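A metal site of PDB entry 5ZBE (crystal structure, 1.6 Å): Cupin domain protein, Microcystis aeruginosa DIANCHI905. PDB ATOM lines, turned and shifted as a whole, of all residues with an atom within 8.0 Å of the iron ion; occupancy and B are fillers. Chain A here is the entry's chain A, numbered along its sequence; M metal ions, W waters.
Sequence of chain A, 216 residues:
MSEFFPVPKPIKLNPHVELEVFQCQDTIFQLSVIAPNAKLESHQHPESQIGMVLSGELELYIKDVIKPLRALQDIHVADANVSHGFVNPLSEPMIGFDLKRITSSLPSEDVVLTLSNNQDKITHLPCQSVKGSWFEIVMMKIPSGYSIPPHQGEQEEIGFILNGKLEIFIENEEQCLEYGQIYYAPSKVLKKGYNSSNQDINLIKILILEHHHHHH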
ATOM      1  N   GLN A  30     -28.118 -24.169  -5.340  1.00  0.00           N
ATOM      2  CA  GLN A  30     -29.333 -23.699  -4.704  1.00  0.00           C
ATOM      3  C   GLN A  30     -30.546 -24.571  -4.907  1.00  0.00           C
ATOM      4  O   GLN A  30     -30.723 -25.144  -5.933  1.00  0.00           O
ATOM      5  CB  GLN A  30     -29.600 -22.278  -5.118  1.00  0.00           C
ATOM      6  CG  GLN A  30     -30.106 -22.125  -6.485  1.00  0.00           C
ATOM      7  CD  GLN A  30     -30.247 -20.673  -6.891  1.00  0.00           C
ATOM      8  OE1 GLN A  30     -29.553 -19.787  -6.403  1.00  0.00           O
ATOM      9  NE2 GLN A  30     -31.138 -20.439  -7.801  1.00  0.00           N
ATOM     10  N   LEU A  40     -39.369 -17.588 -13.603  1.00  0.00           N
ATOM     11  CA  LEU A  40     -38.093 -17.049 -13.245  1.00  0.00           C
ATOM     12  C   LEU A  40     -37.644 -16.353 -14.545  1.00  0.00           C
ATOM     13  O   LEU A  40     -37.407 -17.002 -15.558  1.00  0.00           O
ATOM     14  CB  LEU A  40     -37.162 -18.165 -12.779  1.00  0.00           C
ATOM     15  CG  LEU A  40     -35.863 -17.745 -12.107  1.00  0.00           C
ATOM     16  CD1 LEU A  40     -36.132 -16.996 -10.823  1.00  0.00           C
ATOM     17  CD2 LEU A  40     -34.986 -18.971 -11.857  1.00  0.00           C
ATOM     18  N   GLU A  41     -37.618 -15.020 -14.531  1.00  0.00           N
ATOM     19  CA  GLU A  41     -37.464 -14.249 -15.781  1.00  0.00           C
ATOM     20  C   GLU A  41     -36.075 -14.499 -16.397  1.00  0.00           C
ATOM     21  O   GLU A  41     -35.124 -14.829 -15.685  1.00  0.00           O
ATOM     22  CB  GLU A  41     -37.744 -12.756 -15.558  1.00  0.00           C
ATOM     23  CG  GLU A  41     -38.057 -11.969 -16.834  1.00  0.00           C
ATOM     24  CD  GLU A  41     -39.532 -11.895 -17.205  1.00  0.00           C
ATOM     25  OE1 GLU A  41     -40.354 -11.510 -16.358  1.00  0.00           O
ATOM     26  OE2 GLU A  41     -39.902 -12.185 -18.372  1.00  0.00           O
ATOM     27  N   SER A  42     -35.977 -14.384 -17.717  1.00  0.00           N
ATOM     28  CA  SER A  42     -34.737 -14.723 -18.425  1.00  0.00           C
ATOM     29  C   SER A  42     -33.585 -13.826 -18.029  1.00  0.00           C
ATOM     30  O   SER A  42     -33.779 -12.631 -17.752  1.00  0.00           O
ATOM     31  CB  SER A  42     -34.920 -14.689 -19.943  1.00  0.00           C
ATOM     32  OG  SER A  42     -35.589 -15.859 -20.363  1.00  0.00           O
ATOM     33  N   HIS A  43     -32.394 -14.397 -17.954  1.00  0.00           N
ATOM     34  CA  HIS A  43     -31.208 -13.626 -17.645  1.00  0.00           C
ATOM     35  C   HIS A  43     -29.980 -14.301 -18.175  1.00  0.00           C
ATOM     36  O   HIS A  43     -30.065 -15.393 -18.715  1.00  0.00           O
ATOM     37  CB  HIS A  43     -31.083 -13.350 -16.149  1.00  0.00           C
ATOM     38  CG  HIS A  43     -30.847 -14.569 -15.317  1.00  0.00           C
ATOM     39  ND1 HIS A  43     -31.130 -14.595 -13.975  1.00  0.00           N
ATOM     40  CD2 HIS A  43     -30.331 -15.777 -15.615  1.00  0.00           C
ATOM     41  CE1 HIS A  43     -30.819 -15.782 -13.482  1.00  0.00           C
ATOM     42  NE2 HIS A  43     -30.332 -16.510 -14.461  1.00  0.00           N
ATOM     43  N   GLN A  44     -28.836 -13.651 -18.014  1.00  0.00           N
ATOM     44  CA  GLN A  44     -27.565 -14.284 -18.313  1.00  0.00           C
ATOM     45  C   GLN A  44     -26.557 -13.931 -17.242  1.00  0.00           C
ATOM     46  O   GLN A  44     -26.709 -12.923 -16.546  1.00  0.00           O
ATOM     47  CB  GLN A  44     -27.061 -13.877 -19.706  1.00  0.00           C
ATOM     48  CG  GLN A  44     -26.821 -12.396 -19.898  1.00  0.00           C
ATOM     49  CD  GLN A  44     -26.881 -11.998 -21.381  1.00  0.00           C
ATOM     50  OE1 GLN A  44     -27.775 -11.256 -21.792  1.00  0.00           O
ATOM     51  NE2 GLN A  44     -25.962 -12.528 -22.180  1.00  0.00           N
ATOM     52  N   HIS A  45     -25.558 -14.788 -17.106  1.00  0.00           N
ATOM     53  CA  HIS A  45     -24.466 -14.572 -16.161  1.00  0.00           C
ATOM     54  C   HIS A  45     -23.234 -15.366 -16.586  1.00  0.00           C
ATOM     55  O   HIS A  45     -23.353 -16.363 -17.313  1.00  0.00           O
ATOM     56  CB  HIS A  45     -24.900 -14.978 -14.738  1.00  0.00           C
ATOM     57  CG  HIS A  45     -25.796 -16.175 -14.669  1.00  0.00           C
ATOM     58  ND1 HIS A  45     -25.372 -17.450 -14.962  1.00  0.00           N
ATOM     59  CD2 HIS A  45     -27.093 -16.287 -14.287  1.00  0.00           C
ATOM     60  CE1 HIS A  45     -26.362 -18.304 -14.797  1.00  0.00           C
ATOM     61  NE2 HIS A  45     -27.419 -17.619 -14.365  1.00  0.00           N
ATOM     62  N   GLU A  47     -21.275 -17.339 -14.968  1.00  0.00           N
ATOM     63  CA  GLU A  47     -21.267 -18.735 -14.495  1.00  0.00           C
ATOM     64  C   GLU A  47     -22.084 -19.611 -15.417  1.00  0.00           C
ATOM     65  O   GLU A  47     -23.167 -19.226 -15.855  1.00  0.00           O
ATOM     66  CB  GLU A  47     -21.857 -18.854 -13.100  1.00  0.00           C
ATOM     67  CG  GLU A  47     -21.139 -18.025 -12.044  1.00  0.00           C
ATOM     68  CD  GLU A  47     -21.742 -16.629 -11.831  1.00  0.00           C
ATOM     69  OE1 GLU A  47     -22.423 -16.093 -12.720  1.00  0.00           O
ATOM     70  OE2 GLU A  47     -21.516 -16.061 -10.755  1.00  0.00           O
ATOM     71  N   SER A  48     -21.561 -20.792 -15.700  1.00  0.00           N
ATOM     72  CA  SER A  48     -22.309 -21.876 -16.312  1.00  0.00           C
ATOM     73  C   SER A  48     -23.313 -22.402 -15.295  1.00  0.00           C
ATOM     74  O   SER A  48     -23.081 -22.317 -14.092  1.00  0.00           O
ATOM     75  CB  SER A  48     -21.364 -22.985 -16.724  1.00  0.00           C
ATOM     76  OG  SER A  48     -20.472 -22.522 -17.727  1.00  0.00           O
ATOM     77  N   GLN A  49     -24.424 -22.948 -15.776  1.00  0.00           N
ATOM     78  CA  GLN A  49     -25.495 -23.413 -14.886  1.00  0.00           C
ATOM     79  C   GLN A  49     -26.097 -24.714 -15.345  1.00  0.00           C
ATOM     80  O   GLN A  49     -26.308 -24.923 -16.530  1.00  0.00           O
ATOM     81  CB  GLN A  49     -26.588 -22.337 -14.798  1.00  0.00           C
ATOM     82  CG  GLN A  49     -27.735 -22.668 -13.849  1.00  0.00           C
ATOM     83  CD  GLN A  49     -28.819 -21.601 -13.872  1.00  0.00           C
ATOM     84  OE1 GLN A  49     -30.001 -21.889 -14.138  1.00  0.00           O
ATOM     85  NE2 GLN A  49     -28.449 -20.390 -13.620  1.00  0.00           N
ATOM     86  N   ILE A  50     -26.355 -25.601 -14.381  1.00  0.00           N
ATOM     87  CA  ILE A  50     -27.095 -26.829 -14.627  1.00  0.00           C
ATOM     88  C   ILE A  50     -28.112 -26.993 -13.542  1.00  0.00           C
ATOM     89  O   ILE A  50     -27.973 -26.378 -12.485  1.00  0.00           O
ATOM     90  CB  ILE A  50     -26.196 -28.080 -14.670  1.00  0.00           C
ATOM     91  CG1 ILE A  50     -25.407 -28.219 -13.371  1.00  0.00           C
ATOM     92  CG2 ILE A  50     -25.255 -28.012 -15.859  1.00  0.00           C
ATOM     93  CD1 ILE A  50     -24.495 -29.424 -13.343  1.00  0.00           C
ATOM     94  N   HIS A  76     -31.222 -29.138 -17.204  1.00  0.00           N
ATOM     95  CA  HIS A  76     -30.964 -27.991 -18.054  1.00  0.00           C
ATOM     96  C   HIS A  76     -29.520 -27.645 -18.030  1.00  0.00           C
ATOM     97  O   HIS A  76     -28.841 -27.832 -17.035  1.00  0.00           O
ATOM     98  CB  HIS A  76     -31.845 -26.804 -17.687  1.00  0.00           C
ATOM     99  CG  HIS A  76     -31.443 -26.083 -16.460  1.00  0.00           C
ATOM    100  ND1 HIS A  76     -32.040 -26.278 -15.284  1.00  0.00           N
ATOM    101  CD2 HIS A  76     -30.525 -25.092 -16.253  1.00  0.00           C
ATOM    102  CE1 HIS A  76     -31.508 -25.480 -14.386  1.00  0.00           C
ATOM    103  NE2 HIS A  76     -30.585 -24.742 -14.975  1.00  0.00           N
ATOM    104  N   ALA A  78     -27.119 -24.455 -19.188  1.00  0.00           N
ATOM    105  CA  ALA A  78     -26.956 -23.093 -19.713  1.00  0.00           C
ATOM    106  C   ALA A  78     -25.491 -22.736 -19.619  1.00  0.00           C
ATOM    107  O   ALA A  78     -24.963 -22.574 -18.512  1.00  0.00           O
ATOM    108  CB  ALA A  78     -27.775 -22.107 -18.880  1.00  0.00           C
ATOM    109  N   VAL A  82     -25.282 -17.554 -21.649  1.00  0.00           N
ATOM    110  CA  VAL A  82     -26.421 -17.974 -22.448  1.00  0.00           C
ATOM    111  C   VAL A  82     -27.688 -17.548 -21.715  1.00  0.00           C
ATOM    112  O   VAL A  82     -27.870 -17.895 -20.545  1.00  0.00           O
ATOM    113  CB  VAL A  82     -26.434 -19.504 -22.604  1.00  0.00           C
ATOM    114  CG1 VAL A  82     -27.741 -19.972 -23.253  1.00  0.00           C
ATOM    115  CG2 VAL A  82     -25.258 -19.935 -23.476  1.00  0.00           C
ATOM    116  N   SER A  83     -28.552 -16.804 -22.403  1.00  0.00           N
ATOM    117  CA  SER A  83     -29.817 -16.376 -21.801  1.00  0.00           C
ATOM    118  C   SER A  83     -30.707 -17.567 -21.518  1.00  0.00           C
ATOM    119  O   SER A  83     -30.902 -18.431 -22.376  1.00  0.00           O
ATOM    120  CB  SER A  83     -30.548 -15.398 -22.727  1.00  0.00           C
ATOM    121  OG  SER A  83     -29.744 -14.278 -22.972  1.00  0.00           O
ATOM    122  N   HIS A  84     -31.242 -17.628 -20.300  1.00  0.00           N
ATOM    123  CA  HIS A  84     -32.158 -18.704 -19.911  1.00  0.00           C
ATOM    124  C   HIS A  84     -33.185 -18.205 -18.910  1.00  0.00           C
ATOM    125  O   HIS A  84     -32.866 -17.381 -18.050  1.00  0.00           O
ATOM    126  CB  HIS A  84     -31.401 -19.884 -19.290  1.00  0.00           C
ATOM    127  CG  HIS A  84     -30.504 -19.470 -18.172  1.00  0.00           C
ATOM    128  ND1 HIS A  84     -29.294 -18.840 -18.388  1.00  0.00           N
ATOM    129  CD2 HIS A  84     -30.656 -19.535 -16.835  1.00  0.00           C
ATOM    130  CE1 HIS A  84     -28.727 -18.583 -17.230  1.00  0.00           C
ATOM    131  NE2 HIS A  84     -29.532 -18.988 -16.268  1.00  0.00           N
ATOM    132  N   GLY A  85     -34.392 -18.740 -19.017  1.00  0.00           N
ATOM    133  CA  GLY A  85     -35.479 -18.428 -18.084  1.00  0.00           C
ATOM    134  C   GLY A  85     -36.359 -19.646 -17.973  1.00  0.00           C
ATOM    135  O   GLY A  85     -36.150 -20.638 -18.695  1.00  0.00           O
ATOM    136  N   PHE A  86     -37.318 -19.586 -17.063  1.00  0.00           N
ATOM    137  CA  PHE A  86     -38.183 -20.704 -16.777  1.00  0.00           C
ATOM    138  C   PHE A  86     -39.629 -20.303 -16.547  1.00  0.00           C
ATOM    139  O   PHE A  86     -39.902 -19.234 -16.004  1.00  0.00           O
ATOM    140  CB  PHE A  86     -37.689 -21.377 -15.488  1.00  0.00           C
ATOM    141  CG  PHE A  86     -36.267 -21.856 -15.573  1.00  0.00           C
ATOM    142  CD1 PHE A  86     -35.982 -23.142 -16.030  1.00  0.00           C
ATOM    143  CD2 PHE A  86     -35.211 -21.032 -15.180  1.00  0.00           C
ATOM    144  CE1 PHE A  86     -34.675 -23.603 -16.069  1.00  0.00           C
ATOM    145  CE2 PHE A  86     -33.901 -21.475 -15.240  1.00  0.00           C
ATOM    146  CZ  PHE A  86     -33.630 -22.764 -15.682  1.00  0.00           C
ATOM    147  N   ASP A  98     -30.295 -25.961  -8.773  1.00  0.00           N
ATOM    148  CA  ASP A  98     -29.312 -25.625  -9.789  1.00  0.00           C
ATOM    149  C   ASP A  98     -27.920 -25.387  -9.186  1.00  0.00           C
ATOM    150  O   ASP A  98     -27.782 -25.112  -8.001  1.00  0.00           O
ATOM    151  CB  ASP A  98     -29.758 -24.458 -10.677  1.00  0.00           C
ATOM    152  CG  ASP A  98     -29.810 -23.140  -9.970  1.00  0.00           C
ATOM    153  OD1 ASP A  98     -30.912 -22.730  -9.511  1.00  0.00           O
ATOM    154  OD2 ASP A  98     -28.764 -22.471  -9.921  1.00  0.00           O
ATOM    155  N   LEU A  99     -26.910 -25.525 -10.036  1.00  0.00           N
ATOM    156  CA  LEU A  99     -25.533 -25.245  -9.673  1.00  0.00           C
ATOM    157  C   LEU A  99     -24.989 -24.238 -10.658  1.00  0.00           C
ATOM    158  O   LEU A  99     -25.189 -24.374 -11.798  1.00  0.00           O
ATOM    159  CB  LEU A  99     -24.670 -26.492  -9.839  1.00  0.00           C
ATOM    160  CG  LEU A  99     -24.775 -27.691  -8.947  1.00  0.00           C
ATOM    161  CD1 LEU A  99     -25.971 -28.525  -9.313  1.00  0.00           C
ATOM    162  CD2 LEU A  99     -23.505 -28.468  -9.210  1.00  0.00           C
ATOM    163  N   LYS A 100     -24.271 -23.263 -10.136  1.00  0.00           N
ATOM    164  CA  LYS A 100     -23.606 -22.229 -10.930  1.00  0.00           C
ATOM    165  C   LYS A 100     -22.098 -22.245 -10.626  1.00  0.00           C
ATOM    166  O   LYS A 100     -21.681 -22.274  -9.467  1.00  0.00           O
ATOM    167  CB  LYS A 100     -24.156 -20.836 -10.590  1.00  0.00           C
ATOM    168  CG  LYS A 100     -25.466 -20.468 -11.283  1.00  0.00           C
ATOM    169  CD  LYS A 100     -25.892 -19.052 -10.895  1.00  0.00           C
ATOM    170  CE  LYS A 100     -26.828 -19.028  -9.691  1.00  0.00           C
ATOM    171  NZ  LYS A 100     -28.231 -19.487  -9.996  1.00  0.00           N
HETATM  172 FE    FE M   1     -29.361 -18.491 -14.138  1.00  0.00          FE
HETATM  173  O   HOH W   1     -31.271 -19.298 -13.699  1.00  0.00           O
HETATM  174  O   HOH W   2     -29.331 -18.131 -12.073  1.00  0.00           O
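Four residues have an atom within 4 Å of the iron ion: His 43, His 45, Gln 49 and His 84.
A ring nitrogen (ND1) of His 45 sits at hydrogen-bond distance from the backbone carbonyl oxygen (O) of Glu 47, at 3.0 Å.
O of Ala 78 is in hydrogen-bond range of N of Gln 49, 2.8 Å away.
OE1 of Gln 49 sits at hydrogen-bond distance from NE2 of His 76 (3.0 Å).
O of Val 82 sits at hydrogen-bond distance from ND1 of His 84, at 2.8 Å.
The iron ion is bound by water W2 (2.1 Å), water W1 (2.1 Å), NE2 of His 45 (2.1 Å), NE2 of Gln 49 (2.2 Å), NE2 of His 84 (2.2 Å) and NE2 of His 43 (2.2 Å).
The iron ion has six donor atoms within binding distance.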
